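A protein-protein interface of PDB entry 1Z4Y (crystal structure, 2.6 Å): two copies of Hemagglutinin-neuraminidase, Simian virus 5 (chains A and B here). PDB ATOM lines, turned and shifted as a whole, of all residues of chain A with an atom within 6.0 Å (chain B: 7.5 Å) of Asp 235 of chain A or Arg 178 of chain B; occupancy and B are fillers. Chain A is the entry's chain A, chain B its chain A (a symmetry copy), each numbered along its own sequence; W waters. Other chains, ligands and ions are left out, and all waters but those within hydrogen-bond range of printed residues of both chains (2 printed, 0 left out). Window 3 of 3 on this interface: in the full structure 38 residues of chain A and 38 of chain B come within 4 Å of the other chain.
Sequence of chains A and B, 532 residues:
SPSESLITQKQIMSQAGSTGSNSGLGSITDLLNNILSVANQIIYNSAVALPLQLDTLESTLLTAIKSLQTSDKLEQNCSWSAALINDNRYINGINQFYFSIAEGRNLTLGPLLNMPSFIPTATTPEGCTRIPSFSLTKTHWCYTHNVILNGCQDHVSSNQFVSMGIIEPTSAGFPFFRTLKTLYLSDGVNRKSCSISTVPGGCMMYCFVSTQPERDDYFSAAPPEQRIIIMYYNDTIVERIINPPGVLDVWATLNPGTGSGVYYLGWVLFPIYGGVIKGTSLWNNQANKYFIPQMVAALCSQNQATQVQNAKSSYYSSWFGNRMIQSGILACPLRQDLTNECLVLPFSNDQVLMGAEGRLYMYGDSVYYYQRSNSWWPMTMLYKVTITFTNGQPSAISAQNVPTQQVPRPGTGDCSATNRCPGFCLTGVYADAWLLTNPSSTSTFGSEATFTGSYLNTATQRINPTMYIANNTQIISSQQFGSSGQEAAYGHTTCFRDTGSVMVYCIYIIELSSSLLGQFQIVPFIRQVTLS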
ATOM      1  N   LYS A 181      17.629   8.814 -21.225  1.00  0.00           N
ATOM      2  CA  LYS A 181      16.410   8.606 -21.999  1.00  0.00           C
ATOM      3  C   LYS A 181      16.303   9.690 -23.053  1.00  0.00           C
ATOM      4  O   LYS A 181      16.711  10.822 -22.842  1.00  0.00           O
ATOM      5  CB  LYS A 181      15.155   8.649 -21.121  1.00  0.00           C
ATOM      6  CG  LYS A 181      13.880   8.238 -21.870  1.00  0.00           C
ATOM      7  CD  LYS A 181      12.605   8.521 -21.082  1.00  0.00           C
ATOM      8  CE  LYS A 181      12.565   7.766 -19.771  1.00  0.00           C
ATOM      9  NZ  LYS A 181      12.722   6.294 -19.974  1.00  0.00           N
ATOM     10  N   THR A 182      15.737   9.323 -24.190  1.00  0.00           N
ATOM     11  CA  THR A 182      15.560  10.230 -25.302  1.00  0.00           C
ATOM     12  C   THR A 182      14.119  10.097 -25.791  1.00  0.00           C
ATOM     13  O   THR A 182      13.497   9.050 -25.618  1.00  0.00           O
ATOM     14  CB  THR A 182      16.566   9.858 -26.409  1.00  0.00           C
ATOM     15  OG1 THR A 182      17.609  10.835 -26.441  1.00  0.00           O
ATOM     16  CG2 THR A 182      15.908   9.754 -27.752  1.00  0.00           C
ATOM     17  N   LEU A 183      13.581  11.167 -26.365  1.00  0.00           N
ATOM     18  CA  LEU A 183      12.219  11.156 -26.890  1.00  0.00           C
ATOM     19  C   LEU A 183      12.155  12.087 -28.078  1.00  0.00           C
ATOM     20  O   LEU A 183      12.842  13.103 -28.115  1.00  0.00           O
ATOM     21  CB  LEU A 183      11.204  11.640 -25.851  1.00  0.00           C
ATOM     22  CG  LEU A 183      11.108  10.939 -24.502  1.00  0.00           C
ATOM     23  CD1 LEU A 183      12.097  11.567 -23.521  1.00  0.00           C
ATOM     24  CD2 LEU A 183       9.698  11.088 -23.966  1.00  0.00           C
ATOM     25  N   TYR A 184      11.323  11.750 -29.050  1.00  0.00           N
ATOM     26  CA  TYR A 184      11.180  12.594 -30.226  1.00  0.00           C
ATOM     27  C   TYR A 184       9.692  12.723 -30.509  1.00  0.00           C
ATOM     28  O   TYR A 184       9.073  11.794 -31.017  1.00  0.00           O
ATOM     29  CB  TYR A 184      11.915  11.961 -31.416  1.00  0.00           C
ATOM     30  CG  TYR A 184      12.095  12.861 -32.620  1.00  0.00           C
ATOM     31  CD1 TYR A 184      12.480  14.201 -32.474  1.00  0.00           C
ATOM     32  CD2 TYR A 184      11.927  12.359 -33.914  1.00  0.00           C
ATOM     33  CE1 TYR A 184      12.694  15.012 -33.585  1.00  0.00           C
ATOM     34  CE2 TYR A 184      12.137  13.159 -35.032  1.00  0.00           C
ATOM     35  CZ  TYR A 184      12.522  14.484 -34.864  1.00  0.00           C
ATOM     36  OH  TYR A 184      12.736  15.269 -35.976  1.00  0.00           O
ATOM     37  N   TYR A 232       7.713  11.032 -17.728  1.00  0.00           N
ATOM     38  CA  TYR A 232       8.356  10.409 -16.584  1.00  0.00           C
ATOM     39  C   TYR A 232       9.515   9.518 -16.983  1.00  0.00           C
ATOM     40  O   TYR A 232       9.536   8.941 -18.070  1.00  0.00           O
ATOM     41  CB  TYR A 232       7.326   9.635 -15.753  1.00  0.00           C
ATOM     42  CG  TYR A 232       6.312  10.540 -15.098  1.00  0.00           C
ATOM     43  CD1 TYR A 232       6.642  11.264 -13.955  1.00  0.00           C
ATOM     44  CD2 TYR A 232       5.021  10.688 -15.629  1.00  0.00           C
ATOM     45  CE1 TYR A 232       5.709  12.112 -13.342  1.00  0.00           C
ATOM     46  CE2 TYR A 232       4.076  11.542 -15.028  1.00  0.00           C
ATOM     47  CZ  TYR A 232       4.425  12.248 -13.886  1.00  0.00           C
ATOM     48  OH  TYR A 232       3.503  13.084 -13.266  1.00  0.00           O
ATOM     49  N   TYR A 233      10.487   9.424 -16.090  1.00  0.00           N
ATOM     50  CA  TYR A 233      11.651   8.604 -16.336  1.00  0.00           C
ATOM     51  C   TYR A 233      11.249   7.136 -16.447  1.00  0.00           C
ATOM     52  O   TYR A 233      12.010   6.320 -16.952  1.00  0.00           O
ATOM     53  CB  TYR A 233      12.664   8.801 -15.213  1.00  0.00           C
ATOM     54  CG  TYR A 233      13.936   8.011 -15.398  1.00  0.00           C
ATOM     55  CD1 TYR A 233      14.805   8.272 -16.471  1.00  0.00           C
ATOM     56  CD2 TYR A 233      14.282   7.004 -14.499  1.00  0.00           C
ATOM     57  CE1 TYR A 233      15.980   7.548 -16.628  1.00  0.00           C
ATOM     58  CE2 TYR A 233      15.456   6.277 -14.651  1.00  0.00           C
ATOM     59  CZ  TYR A 233      16.292   6.555 -15.710  1.00  0.00           C
ATOM     60  OH  TYR A 233      17.450   5.843 -15.827  1.00  0.00           O
ATOM     61  N   ASN A 234      10.049   6.793 -15.977  1.00  0.00           N
ATOM     62  CA  ASN A 234       9.574   5.412 -16.077  1.00  0.00           C
ATOM     63  C   ASN A 234       8.866   5.231 -17.403  1.00  0.00           C
ATOM     64  O   ASN A 234       8.138   4.285 -17.613  1.00  0.00           O
ATOM     65  CB  ASN A 234       8.627   5.036 -14.931  1.00  0.00           C
ATOM     66  CG  ASN A 234       7.354   5.840 -14.935  1.00  0.00           C
ATOM     67  OD1 ASN A 234       6.985   6.461 -15.937  1.00  0.00           O
ATOM     68  ND2 ASN A 234       6.665   5.809 -13.788  1.00  0.00           N
ATOM     69  N   ASP A 235       9.111   6.182 -18.289  1.00  0.00           N
ATOM     70  CA  ASP A 235       8.596   6.216 -19.648  1.00  0.00           C
ATOM     71  C   ASP A 235       7.102   6.425 -19.892  1.00  0.00           C
ATOM     72  O   ASP A 235       6.599   6.110 -20.965  1.00  0.00           O
ATOM     73  CB  ASP A 235       9.089   5.003 -20.443  1.00  0.00           C
ATOM     74  CG  ASP A 235       9.760   5.416 -21.764  1.00  0.00           C
ATOM     75  OD1 ASP A 235      10.730   6.209 -21.714  1.00  0.00           O
ATOM     76  OD2 ASP A 235       9.320   4.963 -22.848  1.00  0.00           O
ATOM     77  N   THR A 236       6.392   6.965 -18.911  1.00  0.00           N
ATOM     78  CA  THR A 236       4.982   7.272 -19.090  1.00  0.00           C
ATOM     79  C   THR A 236       4.964   8.684 -19.670  1.00  0.00           C
ATOM     80  O   THR A 236       5.839   9.490 -19.363  1.00  0.00           O
ATOM     81  CB  THR A 236       4.226   7.303 -17.749  1.00  0.00           C
ATOM     82  OG1 THR A 236       3.969   5.964 -17.318  1.00  0.00           O
ATOM     83  CG2 THR A 236       2.905   8.050 -17.884  1.00  0.00           C
ATOM     84  N   ILE A 237       3.986   8.978 -20.517  1.00  0.00           N
ATOM     85  CA  ILE A 237       3.874  10.299 -21.107  1.00  0.00           C
ATOM     86  C   ILE A 237       2.430  10.747 -21.041  1.00  0.00           C
ATOM     87  O   ILE A 237       1.522  10.028 -21.457  1.00  0.00           O
ATOM     88  CB  ILE A 237       4.335  10.316 -22.568  1.00  0.00           C
ATOM     89  CG1 ILE A 237       5.801   9.911 -22.643  1.00  0.00           C
ATOM     90  CG2 ILE A 237       4.160  11.706 -23.153  1.00  0.00           C
ATOM     91  CD1 ILE A 237       6.365   9.931 -24.043  1.00  0.00           C
ATOM     92  N   ILE B  85      13.067  -2.366 -27.050  1.00  0.00           N
ATOM     93  CA  ILE B  85      13.013  -3.162 -28.320  1.00  0.00           C
ATOM     94  C   ILE B  85      12.553  -2.328 -29.524  1.00  0.00           C
ATOM     95  O   ILE B  85      11.738  -1.418 -29.378  1.00  0.00           O
ATOM     96  CB  ILE B  85      12.072  -4.381 -28.165  1.00  0.00           C
ATOM     97  CG1 ILE B  85      12.106  -5.228 -29.440  1.00  0.00           C
ATOM     98  CG2 ILE B  85      10.659  -3.907 -27.855  1.00  0.00           C
ATOM     99  CD1 ILE B  85      11.271  -6.468 -29.384  1.00  0.00           C
ATOM    100  N   ASN B  86      13.068  -2.647 -30.711  1.00  0.00           N
ATOM    101  CA  ASN B  86      12.706  -1.906 -31.919  1.00  0.00           C
ATOM    102  C   ASN B  86      11.220  -1.980 -32.228  1.00  0.00           C
ATOM    103  O   ASN B  86      10.525  -2.898 -31.799  1.00  0.00           O
ATOM    104  CB  ASN B  86      13.490  -2.410 -33.141  1.00  0.00           C
ATOM    105  CG  ASN B  86      14.986  -2.155 -33.032  1.00  0.00           C
ATOM    106  OD1 ASN B  86      15.415  -1.120 -32.529  1.00  0.00           O
ATOM    107  ND2 ASN B  86      15.785  -3.094 -33.526  1.00  0.00           N
ATOM    108  N   PRO B 116      17.480  13.265 -35.863  1.00  0.00           N
ATOM    109  CA  PRO B 116      18.382  13.719 -34.800  1.00  0.00           C
ATOM    110  C   PRO B 116      19.526  12.708 -34.715  1.00  0.00           C
ATOM    111  O   PRO B 116      19.285  11.505 -34.645  1.00  0.00           O
ATOM    112  CB  PRO B 116      17.501  13.682 -33.553  1.00  0.00           C
ATOM    113  CG  PRO B 116      16.129  13.923 -34.101  1.00  0.00           C
ATOM    114  CD  PRO B 116      16.118  13.060 -35.339  1.00  0.00           C
ATOM    115  N   PHE B 118      22.356  10.394 -33.266  1.00  0.00           N
ATOM    116  CA  PHE B 118      22.554   9.687 -32.008  1.00  0.00           C
ATOM    117  C   PHE B 118      24.049   9.555 -31.688  1.00  0.00           C
ATOM    118  O   PHE B 118      24.436   8.884 -30.731  1.00  0.00           O
ATOM    119  CB  PHE B 118      21.880   8.303 -32.078  1.00  0.00           C
ATOM    120  CG  PHE B 118      22.430   7.411 -33.153  1.00  0.00           C
ATOM    121  CD1 PHE B 118      23.530   6.603 -32.906  1.00  0.00           C
ATOM    122  CD2 PHE B 118      21.869   7.410 -34.427  1.00  0.00           C
ATOM    123  CE1 PHE B 118      24.063   5.808 -33.911  1.00  0.00           C
ATOM    124  CE2 PHE B 118      22.396   6.619 -35.438  1.00  0.00           C
ATOM    125  CZ  PHE B 118      23.493   5.817 -35.185  1.00  0.00           C
ATOM    126  N   TRP B 141      20.025  -1.618 -31.124  1.00  0.00           N
ATOM    127  CA  TRP B 141      21.330  -1.275 -31.688  1.00  0.00           C
ATOM    128  C   TRP B 141      22.328  -0.806 -30.637  1.00  0.00           C
ATOM    129  O   TRP B 141      21.944  -0.310 -29.586  1.00  0.00           O
ATOM    130  CB  TRP B 141      21.207  -0.187 -32.759  1.00  0.00           C
ATOM    131  CG  TRP B 141      20.529   1.083 -32.308  1.00  0.00           C
ATOM    132  CD1 TRP B 141      19.233   1.426 -32.525  1.00  0.00           C
ATOM    133  CD2 TRP B 141      21.115   2.176 -31.581  1.00  0.00           C
ATOM    134  NE1 TRP B 141      18.972   2.657 -31.986  1.00  0.00           N
ATOM    135  CE2 TRP B 141      20.106   3.141 -31.402  1.00  0.00           C
ATOM    136  CE3 TRP B 141      22.392   2.431 -31.066  1.00  0.00           C
ATOM    137  CZ2 TRP B 141      20.333   4.351 -30.724  1.00  0.00           C
ATOM    138  CZ3 TRP B 141      22.621   3.636 -30.388  1.00  0.00           C
ATOM    139  CH2 TRP B 141      21.595   4.578 -30.226  1.00  0.00           C
ATOM    140  N   SER B 163      26.770   3.806 -26.588  1.00  0.00           N
ATOM    141  CA  SER B 163      25.376   4.206 -26.707  1.00  0.00           C
ATOM    142  C   SER B 163      24.545   2.976 -27.078  1.00  0.00           C
ATOM    143  O   SER B 163      25.072   2.011 -27.630  1.00  0.00           O
ATOM    144  CB  SER B 163      25.282   5.249 -27.821  1.00  0.00           C
ATOM    145  OG  SER B 163      24.187   6.113 -27.661  1.00  0.00           O
ATOM    146  N   MET B 164      23.253   2.992 -26.775  1.00  0.00           N
ATOM    147  CA  MET B 164      22.400   1.871 -27.152  1.00  0.00           C
ATOM    148  C   MET B 164      20.936   2.290 -27.182  1.00  0.00           C
ATOM    149  O   MET B 164      20.502   3.135 -26.399  1.00  0.00           O
ATOM    150  CB  MET B 164      22.600   0.668 -26.217  1.00  0.00           C
ATOM    151  CG  MET B 164      22.046   0.803 -24.817  1.00  0.00           C
ATOM    152  SD  MET B 164      22.295  -0.747 -23.884  1.00  0.00           S
ATOM    153  CE  MET B 164      24.049  -0.765 -23.650  1.00  0.00           C
ATOM    154  N   GLY B 165      20.182   1.709 -28.106  1.00  0.00           N
ATOM    155  CA  GLY B 165      18.787   2.067 -28.210  1.00  0.00           C
ATOM    156  C   GLY B 165      18.005   1.259 -29.219  1.00  0.00           C
ATOM    157  O   GLY B 165      18.393   0.150 -29.592  1.00  0.00           O
ATOM    158  N   ILE B 166      16.906   1.848 -29.675  1.00  0.00           N
ATOM    159  CA  ILE B 166      16.001   1.208 -30.614  1.00  0.00           C
ATOM    160  C   ILE B 166      15.679   2.119 -31.795  1.00  0.00           C
ATOM    161  O   ILE B 166      16.029   3.300 -31.798  1.00  0.00           O
ATOM    162  CB  ILE B 166      14.678   0.879 -29.918  1.00  0.00           C
ATOM    163  CG1 ILE B 166      13.990   2.191 -29.518  1.00  0.00           C
ATOM    164  CG2 ILE B 166      14.934   0.027 -28.679  1.00  0.00           C
ATOM    165  CD1 ILE B 166      12.641   2.026 -28.906  1.00  0.00           C
ATOM    166  N   ILE B 167      14.988   1.561 -32.786  1.00  0.00           N
ATOM    167  CA  ILE B 167      14.590   2.312 -33.969  1.00  0.00           C
ATOM    168  C   ILE B 167      13.074   2.448 -33.947  1.00  0.00           C
ATOM    169  O   ILE B 167      12.370   1.496 -33.627  1.00  0.00           O
ATOM    170  CB  ILE B 167      14.980   1.583 -35.278  1.00  0.00           C
ATOM    171  CG1 ILE B 167      16.474   1.272 -35.294  1.00  0.00           C
ATOM    172  CG2 ILE B 167      14.634   2.450 -36.474  1.00  0.00           C
ATOM    173  CD1 ILE B 167      16.900   0.429 -36.483  1.00  0.00           C
ATOM    174  N   GLU B 168      12.573   3.631 -34.273  1.00  0.00           N
ATOM    175  CA  GLU B 168      11.136   3.857 -34.307  1.00  0.00           C
ATOM    176  C   GLU B 168      10.823   4.879 -35.382  1.00  0.00           C
ATOM    177  O   GLU B 168      11.597   5.797 -35.623  1.00  0.00           O
ATOM    178  CB  GLU B 168      10.621   4.356 -32.962  1.00  0.00           C
ATOM    179  CG  GLU B 168      11.183   5.682 -32.541  1.00  0.00           C
ATOM    180  CD  GLU B 168      10.490   6.225 -31.311  1.00  0.00           C
ATOM    181  OE1 GLU B 168      10.286   5.445 -30.351  1.00  0.00           O
ATOM    182  OE2 GLU B 168      10.159   7.432 -31.301  1.00  0.00           O
ATOM    183  N   PRO B 175      13.011   6.550 -40.106  1.00  0.00           N
ATOM    184  CA  PRO B 175      13.542   6.213 -38.782  1.00  0.00           C
ATOM    185  C   PRO B 175      14.055   7.317 -37.878  1.00  0.00           C
ATOM    186  O   PRO B 175      14.334   8.436 -38.297  1.00  0.00           O
ATOM    187  CB  PRO B 175      14.663   5.218 -39.093  1.00  0.00           C
ATOM    188  CG  PRO B 175      14.316   4.684 -40.430  1.00  0.00           C
ATOM    189  CD  PRO B 175      13.825   5.903 -41.147  1.00  0.00           C
ATOM    190  N   PHE B 176      14.175   6.945 -36.611  1.00  0.00           N
ATOM    191  CA  PHE B 176      14.698   7.800 -35.573  1.00  0.00           C
ATOM    192  C   PHE B 176      15.372   6.851 -34.606  1.00  0.00           C
ATOM    193  O   PHE B 176      14.708   6.058 -33.953  1.00  0.00           O
ATOM    194  CB  PHE B 176      13.592   8.563 -34.847  1.00  0.00           C
ATOM    195  CG  PHE B 176      14.002   9.063 -33.484  1.00  0.00           C
ATOM    196  CD1 PHE B 176      15.205   9.741 -33.310  1.00  0.00           C
ATOM    197  CD2 PHE B 176      13.204   8.830 -32.373  1.00  0.00           C
ATOM    198  CE1 PHE B 176      15.606  10.189 -32.046  1.00  0.00           C
ATOM    199  CE2 PHE B 176      13.595   9.276 -31.103  1.00  0.00           C
ATOM    200  CZ  PHE B 176      14.799   9.952 -30.943  1.00  0.00           C
ATOM    201  N   PHE B 177      16.694   6.913 -34.541  1.00  0.00           N
ATOM    202  CA  PHE B 177      17.433   6.058 -33.639  1.00  0.00           C
ATOM    203  C   PHE B 177      17.334   6.650 -32.251  1.00  0.00           C
ATOM    204  O   PHE B 177      17.993   7.630 -31.920  1.00  0.00           O
ATOM    205  CB  PHE B 177      18.877   5.925 -34.115  1.00  0.00           C
ATOM    206  CG  PHE B 177      19.012   5.084 -35.347  1.00  0.00           C
ATOM    207  CD1 PHE B 177      18.412   5.480 -36.540  1.00  0.00           C
ATOM    208  CD2 PHE B 177      19.665   3.863 -35.305  1.00  0.00           C
ATOM    209  CE1 PHE B 177      18.465   4.669 -37.667  1.00  0.00           C
ATOM    210  CE2 PHE B 177      19.721   3.045 -36.434  1.00  0.00           C
ATOM    211  CZ  PHE B 177      19.117   3.448 -37.612  1.00  0.00           C
ATOM    212  N   ARG B 178      16.465   6.043 -31.453  1.00  0.00           N
ATOM    213  CA  ARG B 178      16.199   6.477 -30.093  1.00  0.00           C
ATOM    214  C   ARG B 178      17.169   5.881 -29.074  1.00  0.00           C
ATOM    215  O   ARG B 178      17.173   4.673 -28.831  1.00  0.00           O
ATOM    216  CB  ARG B 178      14.769   6.096 -29.722  1.00  0.00           C
ATOM    217  CG  ARG B 178      14.286   6.758 -28.463  1.00  0.00           C
ATOM    218  CD  ARG B 178      13.022   6.142 -27.959  1.00  0.00           C
ATOM    219  NE  ARG B 178      12.646   6.732 -26.684  1.00  0.00           N
ATOM    220  CZ  ARG B 178      11.685   6.259 -25.904  1.00  0.00           C
ATOM    221  NH1 ARG B 178      11.011   5.186 -26.276  1.00  0.00           N
ATOM    222  NH2 ARG B 178      11.401   6.852 -24.754  1.00  0.00           N
ATOM    223  N   THR B 179      17.987   6.744 -28.481  1.00  0.00           N
ATOM    224  CA  THR B 179      18.962   6.323 -27.484  1.00  0.00           C
ATOM    225  C   THR B 179      18.249   6.085 -26.175  1.00  0.00           C
ATOM    226  O   THR B 179      17.534   6.964 -25.695  1.00  0.00           O
ATOM    227  CB  THR B 179      20.022   7.407 -27.233  1.00  0.00           C
ATOM    228  OG1 THR B 179      20.754   7.655 -28.437  1.00  0.00           O
ATOM    229  CG2 THR B 179      20.980   6.965 -26.138  1.00  0.00           C
ATOM    230  N   LEU B 180      18.457   4.906 -25.591  1.00  0.00           N
ATOM    231  CA  LEU B 180      17.825   4.561 -24.327  1.00  0.00           C
ATOM    232  C   LEU B 180      18.814   4.504 -23.164  1.00  0.00           C
ATOM    233  O   LEU B 180      18.410   4.421 -22.008  1.00  0.00           O
ATOM    234  CB  LEU B 180      17.095   3.227 -24.450  1.00  0.00           C
ATOM    235  CG  LEU B 180      15.893   3.210 -25.387  1.00  0.00           C
ATOM    236  CD1 LEU B 180      15.181   1.872 -25.254  1.00  0.00           C
ATOM    237  CD2 LEU B 180      14.951   4.343 -25.039  1.00  0.00           C
ATOM    238  N   LYS B 181      20.105   4.533 -23.472  1.00  0.00           N
ATOM    239  CA  LYS B 181      21.145   4.506 -22.449  1.00  0.00           C
ATOM    240  C   LYS B 181      22.449   4.986 -23.056  1.00  0.00           C
ATOM    241  O   LYS B 181      22.729   4.753 -24.223  1.00  0.00           O
ATOM    242  CB  LYS B 181      21.357   3.099 -21.879  1.00  0.00           C
ATOM    243  CG  LYS B 181      22.298   3.075 -20.667  1.00  0.00           C
ATOM    244  CD  LYS B 181      22.711   1.665 -20.258  1.00  0.00           C
ATOM    245  CE  LYS B 181      21.523   0.814 -19.864  1.00  0.00           C
ATOM    246  NZ  LYS B 181      20.726   1.448 -18.772  1.00  0.00           N
ATOM    247  N   TYR B 233      21.435  -3.675 -20.539  1.00  0.00           N
ATOM    248  CA  TYR B 233      20.458  -2.611 -20.552  1.00  0.00           C
ATOM    249  C   TYR B 233      19.925  -2.365 -19.144  1.00  0.00           C
ATOM    250  O   TYR B 233      19.335  -1.326 -18.876  1.00  0.00           O
ATOM    251  CB  TYR B 233      19.320  -2.970 -21.503  1.00  0.00           C
ATOM    252  CG  TYR B 233      18.263  -1.900 -21.615  1.00  0.00           C
ATOM    253  CD1 TYR B 233      18.558  -0.640 -22.158  1.00  0.00           C
ATOM    254  CD2 TYR B 233      16.960  -2.145 -21.185  1.00  0.00           C
ATOM    255  CE1 TYR B 233      17.576   0.337 -22.269  1.00  0.00           C
ATOM    256  CE2 TYR B 233      15.973  -1.173 -21.293  1.00  0.00           C
ATOM    257  CZ  TYR B 233      16.289   0.054 -21.834  1.00  0.00           C
ATOM    258  OH  TYR B 233      15.299   0.986 -21.950  1.00  0.00           O
HETATM  259  O   HOH W   1       8.986   9.439 -32.982  1.00  0.00           O
HETATM  260  O   HOH W   2       9.917   8.985 -28.705  1.00  0.00           O
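Positions printed for both chains: 181 and 233.
Of chain B, only Arg 178 comes within 4 Å of Asp 235 of chain A.
Of chain A, only Thr 182 and Asp 235 come within 4 Å of Arg 178 of chain B.
Of the printed residues of chain B, Tyr 184 of chain A touches Pro 116 (3.6 Å) and Phe 176 (3.2 Å).
Of the printed residues of chain B, Thr 182 of chain A touches Phe 176 (3.4 Å), Arg 178 (2.7 Å) and Thr 179 (3.1 Å).
Of the printed residues of chain B, Lys 181 of chain A touches Thr 179.
Tyr 233 of chain A touches none of the printed residues of chain B.
The nearest residue of chain B that does not touch Asp 235 of chain A is Leu 180 of chain B (5.7 Å).
Hydrophobic or aromatic side chains of chain B that line the printed part of chain A: Pro 116 and Phe 176.
Along chain B the printed residues that touch a printed residue of chain A span positions 116 to 179.
Hydrophobic or aromatic side chains of chain A that line the printed part of chain B: Tyr 184.
Along chain A the printed residues that touch a printed residue of chain B span positions 181 to 235.
Water W1 lies within hydrogen-bond range of the side-chain carboxylate of Glu 168 of chain B and the backbone carbonyl oxygen of Tyr 184 of chain A.
Water W2 bridges OE2 of Glu 168 of chain B and N of Tyr 184 of chain A.
Among the printed residues, merely in contact across the chains: Tyr 184 of chain A with Phe 176 of chain B, Thr 182 of chain A with Phe 176 of chain B, Tyr 184 of chain A with Pro 116 of chain B and Lys 181 of chain A with Thr 179 of chain B.
NZ of Lys 181 of chain A is in hydrogen-bond range of O of Tyr 233 of chain A, 3.1 Å away.
The side-chain carboxylate (OD1) of Asp 235 of chain A is in salt-bridge range of the side-chain amino group (NZ) of Lys 181 of chain A (2.6 Å).
The backbone carbonyl oxygen (O) of Ile 166 of chain B sits at hydrogen-bond distance from the backbone NH (N) of Arg 178 of chain B, at 2.8 Å.
O of Glu 168 of chain B is in hydrogen-bond range of N of Phe 176 of chain B (3.0 Å).
The guanidinium group (NE) of Arg 178 of chain B lies within hydrogen-bond range of the backbone carbonyl oxygen (O) of Thr 182 of chain A, 2.7 Å away.
N of Thr 182 of chain A lies close to O of Thr 179 of chain B.
OD1 of Asp 235 of chain A is in salt-bridge range of NH2 of Arg 178 of chain B (3.2 Å).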
